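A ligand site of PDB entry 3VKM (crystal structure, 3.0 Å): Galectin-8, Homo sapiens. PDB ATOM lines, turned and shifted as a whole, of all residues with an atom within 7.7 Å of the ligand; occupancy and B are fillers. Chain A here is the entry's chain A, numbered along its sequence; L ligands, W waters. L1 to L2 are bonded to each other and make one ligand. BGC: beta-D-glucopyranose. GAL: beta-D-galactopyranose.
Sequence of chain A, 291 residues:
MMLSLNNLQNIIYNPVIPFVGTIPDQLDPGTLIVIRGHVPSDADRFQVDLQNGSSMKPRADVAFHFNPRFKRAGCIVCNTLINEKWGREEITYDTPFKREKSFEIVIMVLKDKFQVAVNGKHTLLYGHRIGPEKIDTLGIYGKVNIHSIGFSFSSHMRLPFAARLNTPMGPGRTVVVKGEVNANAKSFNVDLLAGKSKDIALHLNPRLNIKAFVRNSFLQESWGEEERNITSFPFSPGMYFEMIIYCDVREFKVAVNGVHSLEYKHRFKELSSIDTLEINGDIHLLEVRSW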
ATOM      1  N   SER A 187      12.394 -13.490  24.107  1.00  0.00           N
ATOM      2  CA  SER A 187      11.363 -12.998  23.219  1.00  0.00           C
ATOM      3  C   SER A 187      11.383 -11.485  23.137  1.00  0.00           C
ATOM      4  O   SER A 187      12.070 -10.813  23.918  1.00  0.00           O
ATOM      5  CB  SER A 187       9.985 -13.434  23.703  1.00  0.00           C
ATOM      6  OG  SER A 187       9.698 -12.779  24.927  1.00  0.00           O
ATOM      7  N   ASN A 189       8.596  -8.071  21.465  1.00  0.00           N
ATOM      8  CA  ASN A 189       7.262  -7.821  20.935  1.00  0.00           C
ATOM      9  C   ASN A 189       7.132  -6.499  20.201  1.00  0.00           C
ATOM     10  O   ASN A 189       7.813  -5.521  20.510  1.00  0.00           O
ATOM     11  CB  ASN A 189       6.254  -7.833  22.085  1.00  0.00           C
ATOM     12  CG  ASN A 189       6.473  -6.683  23.085  1.00  0.00           C
ATOM     13  OD1 ASN A 189       5.698  -6.488  24.018  1.00  0.00           O
ATOM     14  ND2 ASN A 189       7.542  -5.915  22.885  1.00  0.00           N
ATOM     15  N   ASP A 191       3.937  -4.096  19.067  1.00  0.00           N
ATOM     16  CA  ASP A 191       2.488  -3.922  19.174  1.00  0.00           C
ATOM     17  C   ASP A 191       1.925  -2.698  18.460  1.00  0.00           C
ATOM     18  O   ASP A 191       2.560  -1.652  18.404  1.00  0.00           O
ATOM     19  CB  ASP A 191       2.079  -3.800  20.659  1.00  0.00           C
ATOM     20  CG  ASP A 191       2.580  -4.950  21.525  1.00  0.00           C
ATOM     21  OD1 ASP A 191       2.569  -6.104  21.035  1.00  0.00           O
ATOM     22  OD2 ASP A 191       2.961  -4.702  22.689  1.00  0.00           O
ATOM     23  N   ILE A 200      -4.863  -3.138  22.294  1.00  0.00           N
ATOM     24  CA  ILE A 200      -3.767  -3.640  21.487  1.00  0.00           C
ATOM     25  C   ILE A 200      -4.361  -4.367  20.288  1.00  0.00           C
ATOM     26  O   ILE A 200      -4.769  -5.526  20.375  1.00  0.00           O
ATOM     27  CB  ILE A 200      -2.870  -4.596  22.304  1.00  0.00           C
ATOM     28  CG1 ILE A 200      -2.393  -3.896  23.568  1.00  0.00           C
ATOM     29  CG2 ILE A 200      -1.685  -5.033  21.479  1.00  0.00           C
ATOM     30  CD1 ILE A 200      -1.468  -4.746  24.422  1.00  0.00           C
ATOM     31  N   HIS A 203      -0.685  -7.700  18.450  1.00  0.00           N
ATOM     32  CA  HIS A 203       0.420  -8.016  19.333  1.00  0.00           C
ATOM     33  C   HIS A 203       1.206  -9.086  18.621  1.00  0.00           C
ATOM     34  O   HIS A 203       0.751 -10.223  18.493  1.00  0.00           O
ATOM     35  CB  HIS A 203      -0.137  -8.534  20.663  1.00  0.00           C
ATOM     36  CG  HIS A 203       0.918  -8.967  21.640  1.00  0.00           C
ATOM     37  ND1 HIS A 203       1.912  -8.124  22.088  1.00  0.00           N
ATOM     38  CD2 HIS A 203       1.093 -10.145  22.287  1.00  0.00           C
ATOM     39  CE1 HIS A 203       2.649  -8.766  22.983  1.00  0.00           C
ATOM     40  NE2 HIS A 203       2.178  -9.984  23.120  1.00  0.00           N
ATOM     41  N   LEU A 204       2.385  -8.712  18.122  1.00  0.00           N
ATOM     42  CA  LEU A 204       3.259  -9.648  17.441  1.00  0.00           C
ATOM     43  C   LEU A 204       4.311  -9.996  18.463  1.00  0.00           C
ATOM     44  O   LEU A 204       5.133  -9.155  18.844  1.00  0.00           O
ATOM     45  CB  LEU A 204       3.888  -8.990  16.205  1.00  0.00           C
ATOM     46  CG  LEU A 204       2.896  -8.661  15.079  1.00  0.00           C
ATOM     47  CD1 LEU A 204       3.653  -8.074  13.908  1.00  0.00           C
ATOM     48  CD2 LEU A 204       2.157  -9.911  14.656  1.00  0.00           C
ATOM     49  N   ASN A 205       4.305 -11.239  18.914  1.00  0.00           N
ATOM     50  CA  ASN A 205       5.220 -11.647  19.962  1.00  0.00           C
ATOM     51  C   ASN A 205       6.104 -12.841  19.572  1.00  0.00           C
ATOM     52  O   ASN A 205       5.764 -13.983  19.848  1.00  0.00           O
ATOM     53  CB  ASN A 205       4.399 -11.976  21.215  1.00  0.00           C
ATOM     54  CG  ASN A 205       5.248 -12.417  22.396  1.00  0.00           C
ATOM     55  OD1 ASN A 205       4.734 -12.928  23.383  1.00  0.00           O
ATOM     56  ND2 ASN A 205       6.559 -12.209  22.306  1.00  0.00           N
ATOM     57  N   ARG A 207       8.665 -15.479  20.093  1.00  0.00           N
ATOM     58  CA  ARG A 207       9.271 -16.035  21.295  1.00  0.00           C
ATOM     59  C   ARG A 207      10.324 -17.007  20.803  1.00  0.00           C
ATOM     60  O   ARG A 207      10.025 -18.000  20.135  1.00  0.00           O
ATOM     61  CB  ARG A 207       8.222 -16.749  22.155  1.00  0.00           C
ATOM     62  CG  ARG A 207       7.634 -15.877  23.245  1.00  0.00           C
ATOM     63  CD  ARG A 207       6.120 -15.657  23.116  1.00  0.00           C
ATOM     64  NE  ARG A 207       5.356 -16.502  24.042  1.00  0.00           N
ATOM     65  CZ  ARG A 207       4.108 -16.241  24.431  1.00  0.00           C
ATOM     66  NH1 ARG A 207       3.458 -15.172  23.994  1.00  0.00           N
ATOM     67  NH2 ARG A 207       3.507 -17.067  25.273  1.00  0.00           N
ATOM     68  N   ILE A 210      10.776 -20.625  22.934  1.00  0.00           N
ATOM     69  CA  ILE A 210       9.894 -21.724  22.572  1.00  0.00           C
ATOM     70  C   ILE A 210       9.707 -21.881  21.082  1.00  0.00           C
ATOM     71  O   ILE A 210       8.882 -22.684  20.656  1.00  0.00           O
ATOM     72  CB  ILE A 210       8.499 -21.678  23.257  1.00  0.00           C
ATOM     73  CG1 ILE A 210       7.861 -20.291  23.095  1.00  0.00           C
ATOM     74  CG2 ILE A 210       8.650 -22.099  24.708  1.00  0.00           C
ATOM     75  CD1 ILE A 210       6.454 -20.213  23.654  1.00  0.00           C
ATOM     76  N   VAL A 214       3.489 -15.952  18.784  1.00  0.00           N
ATOM     77  CA  VAL A 214       2.163 -15.688  19.334  1.00  0.00           C
ATOM     78  C   VAL A 214       1.662 -14.377  18.782  1.00  0.00           C
ATOM     79  O   VAL A 214       2.362 -13.353  18.784  1.00  0.00           O
ATOM     80  CB  VAL A 214       2.195 -15.592  20.877  1.00  0.00           C
ATOM     81  CG1 VAL A 214       0.785 -15.407  21.410  1.00  0.00           C
ATOM     82  CG2 VAL A 214       2.830 -16.840  21.455  1.00  0.00           C
ATOM     83  N   ARG A 215       0.423 -14.405  18.326  1.00  0.00           N
ATOM     84  CA  ARG A 215      -0.213 -13.242  17.735  1.00  0.00           C
ATOM     85  C   ARG A 215      -1.562 -13.171  18.409  1.00  0.00           C
ATOM     86  O   ARG A 215      -2.280 -14.170  18.516  1.00  0.00           O
ATOM     87  CB  ARG A 215      -0.324 -13.484  16.225  1.00  0.00           C
ATOM     88  CG  ARG A 215       0.908 -14.210  15.726  1.00  0.00           C
ATOM     89  CD  ARG A 215       1.018 -14.212  14.243  1.00  0.00           C
ATOM     90  NE  ARG A 215       0.199 -15.235  13.585  1.00  0.00           N
ATOM     91  CZ  ARG A 215       0.448 -16.538  13.604  1.00  0.00           C
ATOM     92  NH1 ARG A 215       1.499 -17.021  14.262  1.00  0.00           N
ATOM     93  NH2 ARG A 215      -0.340 -17.374  12.953  1.00  0.00           N
ATOM     94  N   ASN A 216      -1.916 -11.984  18.879  1.00  0.00           N
ATOM     95  CA  ASN A 216      -3.168 -11.847  19.602  1.00  0.00           C
ATOM     96  C   ASN A 216      -3.541 -10.390  19.716  1.00  0.00           C
ATOM     97  O   ASN A 216      -2.793  -9.513  19.281  1.00  0.00           O
ATOM     98  CB  ASN A 216      -2.990 -12.436  21.005  1.00  0.00           C
ATOM     99  CG  ASN A 216      -4.280 -12.941  21.606  1.00  0.00           C
ATOM    100  OD1 ASN A 216      -5.355 -12.789  21.035  1.00  0.00           O
ATOM    101  ND2 ASN A 216      -4.172 -13.554  22.786  1.00  0.00           N
ATOM    102  N   SER A 217      -4.710 -10.132  20.292  1.00  0.00           N
ATOM    103  CA  SER A 217      -5.185  -8.763  20.491  1.00  0.00           C
ATOM    104  C   SER A 217      -5.609  -8.599  21.940  1.00  0.00           C
ATOM    105  O   SER A 217      -6.103  -9.529  22.570  1.00  0.00           O
ATOM    106  CB  SER A 217      -6.350  -8.468  19.550  1.00  0.00           C
ATOM    107  OG  SER A 217      -5.897  -8.381  18.221  1.00  0.00           O
ATOM    108  N   PHE A 218      -5.397  -7.394  22.464  1.00  0.00           N
ATOM    109  CA  PHE A 218      -5.758  -7.092  23.840  1.00  0.00           C
ATOM    110  C   PHE A 218      -6.825  -6.003  23.775  1.00  0.00           C
ATOM    111  O   PHE A 218      -6.542  -4.851  23.506  1.00  0.00           O
ATOM    112  CB  PHE A 218      -4.510  -6.582  24.593  1.00  0.00           C
ATOM    113  CG  PHE A 218      -4.696  -6.499  26.074  1.00  0.00           C
ATOM    114  CD1 PHE A 218      -5.070  -7.620  26.810  1.00  0.00           C
ATOM    115  CD2 PHE A 218      -4.506  -5.285  26.746  1.00  0.00           C
ATOM    116  CE1 PHE A 218      -5.251  -7.544  28.193  1.00  0.00           C
ATOM    117  CE2 PHE A 218      -4.686  -5.193  28.123  1.00  0.00           C
ATOM    118  CZ  PHE A 218      -5.066  -6.322  28.855  1.00  0.00           C
ATOM    119  N   TRP A 223      -7.002 -10.465  26.876  1.00  0.00           N
ATOM    120  CA  TRP A 223      -6.328 -11.159  25.785  1.00  0.00           C
ATOM    121  C   TRP A 223      -7.333 -12.069  25.088  1.00  0.00           C
ATOM    122  O   TRP A 223      -8.164 -12.696  25.727  1.00  0.00           O
ATOM    123  CB  TRP A 223      -5.171 -11.997  26.338  1.00  0.00           C
ATOM    124  CG  TRP A 223      -3.945 -11.218  26.636  1.00  0.00           C
ATOM    125  CD1 TRP A 223      -3.282 -11.143  27.821  1.00  0.00           C
ATOM    126  CD2 TRP A 223      -3.198 -10.413  25.705  1.00  0.00           C
ATOM    127  NE1 TRP A 223      -2.166 -10.354  27.697  1.00  0.00           N
ATOM    128  CE2 TRP A 223      -2.090  -9.895  26.404  1.00  0.00           C
ATOM    129  CE3 TRP A 223      -3.356 -10.102  24.351  1.00  0.00           C
ATOM    130  CZ2 TRP A 223      -1.133  -9.068  25.794  1.00  0.00           C
ATOM    131  CZ3 TRP A 223      -2.415  -9.279  23.747  1.00  0.00           C
ATOM    132  CH2 TRP A 223      -1.322  -8.777  24.470  1.00  0.00           C
ATOM    133  N   GLY A 224      -7.241 -12.122  23.759  1.00  0.00           N
ATOM    134  CA  GLY A 224      -8.137 -12.966  22.985  1.00  0.00           C
ATOM    135  C   GLY A 224      -7.568 -14.348  22.758  1.00  0.00           C
ATOM    136  O   GLY A 224      -6.771 -14.848  23.548  1.00  0.00           O
ATOM    137  N   GLU A 225      -8.002 -14.968  21.671  1.00  0.00           N
ATOM    138  CA  GLU A 225      -7.530 -16.300  21.297  1.00  0.00           C
ATOM    139  C   GLU A 225      -6.218 -16.136  20.523  1.00  0.00           C
ATOM    140  O   GLU A 225      -6.152 -15.363  19.573  1.00  0.00           O
ATOM    141  CB  GLU A 225      -8.570 -16.985  20.412  1.00  0.00           C
ATOM    142  CG  GLU A 225      -8.225 -18.419  20.024  1.00  0.00           C
ATOM    143  CD  GLU A 225      -9.143 -18.973  18.942  1.00  0.00           C
ATOM    144  OE1 GLU A 225      -8.915 -20.122  18.496  1.00  0.00           O
ATOM    145  OE2 GLU A 225     -10.091 -18.255  18.542  1.00  0.00           O
ATOM    146  N   GLU A 226      -5.171 -16.840  20.937  1.00  0.00           N
ATOM    147  CA  GLU A 226      -3.890 -16.704  20.264  1.00  0.00           C
ATOM    148  C   GLU A 226      -3.838 -17.357  18.890  1.00  0.00           C
ATOM    149  O   GLU A 226      -4.575 -18.305  18.604  1.00  0.00           O
ATOM    150  CB  GLU A 226      -2.777 -17.273  21.136  1.00  0.00           C
ATOM    151  CG  GLU A 226      -2.783 -16.706  22.535  1.00  0.00           C
ATOM    152  CD  GLU A 226      -1.507 -16.998  23.284  1.00  0.00           C
ATOM    153  OE1 GLU A 226      -1.048 -18.150  23.259  1.00  0.00           O
ATOM    154  OE2 GLU A 226      -0.967 -16.062  23.905  1.00  0.00           O
ATOM    155  N   GLU A 227      -2.971 -16.830  18.029  1.00  0.00           N
ATOM    156  CA  GLU A 227      -2.761 -17.342  16.678  1.00  0.00           C
ATOM    157  C   GLU A 227      -1.281 -17.690  16.556  1.00  0.00           C
ATOM    158  O   GLU A 227      -0.421 -16.798  16.595  1.00  0.00           O
ATOM    159  CB  GLU A 227      -3.149 -16.315  15.631  1.00  0.00           C
ATOM    160  CG  GLU A 227      -4.642 -16.028  15.548  1.00  0.00           C
ATOM    161  CD  GLU A 227      -5.052 -15.470  14.192  1.00  0.00           C
ATOM    162  OE1 GLU A 227      -4.677 -16.084  13.158  1.00  0.00           O
ATOM    163  OE2 GLU A 227      -5.746 -14.436  14.154  1.00  0.00           O
ATOM    164  N   ARG A 228      -0.979 -18.982  16.399  1.00  0.00           N
ATOM    165  CA  ARG A 228       0.408 -19.430  16.318  1.00  0.00           C
ATOM    166  C   ARG A 228       0.769 -20.210  15.050  1.00  0.00           C
ATOM    167  O   ARG A 228       1.957 -20.478  14.813  1.00  0.00           O
ATOM    168  CB  ARG A 228       0.749 -20.314  17.520  1.00  0.00           C
ATOM    169  CG  ARG A 228       0.500 -19.719  18.892  1.00  0.00           C
ATOM    170  CD  ARG A 228       0.923 -20.679  19.969  1.00  0.00           C
ATOM    171  NE  ARG A 228       0.905 -20.053  21.293  1.00  0.00           N
ATOM    172  CZ  ARG A 228       1.461 -20.593  22.375  1.00  0.00           C
ATOM    173  NH1 ARG A 228       2.063 -21.765  22.291  1.00  0.00           N
ATOM    174  NH2 ARG A 228       1.424 -19.951  23.534  1.00  0.00           N
HETATM  175  C2  BGC L   1      -0.312 -18.311  26.755  1.00  0.00           C
HETATM  176  C3  BGC L   1       0.650 -17.132  26.839  1.00  0.00           C
HETATM  177  C4  BGC L   1       0.165 -16.132  27.899  1.00  0.00           C
HETATM  178  C5  BGC L   1      -0.008 -16.874  29.236  1.00  0.00           C
HETATM  179  C6  BGC L   1      -0.524 -15.988  30.353  1.00  0.00           C
HETATM  180  C1  BGC L   1      -0.471 -18.946  28.147  1.00  0.00           C
HETATM  181  O1  BGC L   1      -1.403 -19.965  28.094  1.00  0.00           O
HETATM  182  O2  BGC L   1       0.190 -19.271  25.830  1.00  0.00           O
HETATM  183  O3  BGC L   1       0.726 -16.488  25.575  1.00  0.00           O
HETATM  184  O4  BGC L   1       1.114 -15.061  28.037  1.00  0.00           O
HETATM  185  O5  BGC L   1      -0.933 -17.966  29.079  1.00  0.00           O
HETATM  186  O6  BGC L   1      -1.475 -15.053  29.871  1.00  0.00           O
HETATM  187  C1  GAL L   2       0.710 -13.801  27.633  1.00  0.00           C
HETATM  188  C2  GAL L   2       1.859 -12.805  27.846  1.00  0.00           C
HETATM  189  C3  GAL L   2       1.477 -11.443  27.259  1.00  0.00           C
HETATM  190  C4  GAL L   2       1.132 -11.624  25.778  1.00  0.00           C
HETATM  191  C5  GAL L   2      -0.028 -12.601  25.675  1.00  0.00           C
HETATM  192  C6  GAL L   2      -0.413 -12.843  24.240  1.00  0.00           C
HETATM  193  O2  GAL L   2       2.131 -12.667  29.227  1.00  0.00           O
HETATM  194  O3  GAL L   2       2.567 -10.551  27.393  1.00  0.00           O
HETATM  195  O4  GAL L   2       2.245 -12.168  25.085  1.00  0.00           O
HETATM  196  O5  GAL L   2       0.354 -13.869  26.233  1.00  0.00           O
HETATM  197  O6  GAL L   2      -1.596 -13.614  24.185  1.00  0.00           O
HETATM  198  O   HOH W   1      -3.308 -15.525  27.197  1.00  0.00           O
HETATM  199  O   HOH W   2      -1.103 -23.006  29.423  1.00  0.00           O
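OE2 of Glu 226 is in hydrogen-bond range of O3 of BGC L1.
NH2 of Arg 228 is in hydrogen-bond range of O2 of BGC L1, 2.7 Å away.
The guanidinium group (NH2) of Arg 207 is in hydrogen-bond range of an oxygen (O3) of BGC L1, 2.9 Å away.
The side-chain amide nitrogen (ND2) of Asn 216 lies within hydrogen-bond range of an oxygen (O6) of GAL L2 (2.9 Å).
A ring nitrogen (NE2) of His 203 is in hydrogen-bond range of an oxygen (O4) of GAL L2 (2.9 Å).
An oxygen (O4) of GAL L2 sits at hydrogen-bond distance from the side-chain amide oxygen (OD1) of Asn 205 (3.1 Å).
OE1 of Glu 226 lies within salt-bridge range of NH2 of Arg 228, at 3.1 Å.
The guanidinium group (NH1) of Arg 207 sits at hydrogen-bond distance from the side-chain amide oxygen (OD1) of Asn 205, at 2.7 Å.
N of His 203 is in hydrogen-bond range of O of Asn 216, 2.9 Å away.
The side-chain amide nitrogen (ND2) of Asn 216 sits at hydrogen-bond distance from the backbone carbonyl oxygen (O) of Gly 224, 3.0 Å away.
The side-chain amide oxygen (OD1) of Asn 216 sits close to the backbone carbonyl oxygen (O) of Glu 225 (3.1 Å).
The backbone NH of Asn 205 lies within hydrogen-bond range of the backbone carbonyl oxygen of Val 214 (2.9 Å).
CZ2 of Trp 223 touches C4 of GAL L2 (3.4 Å).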
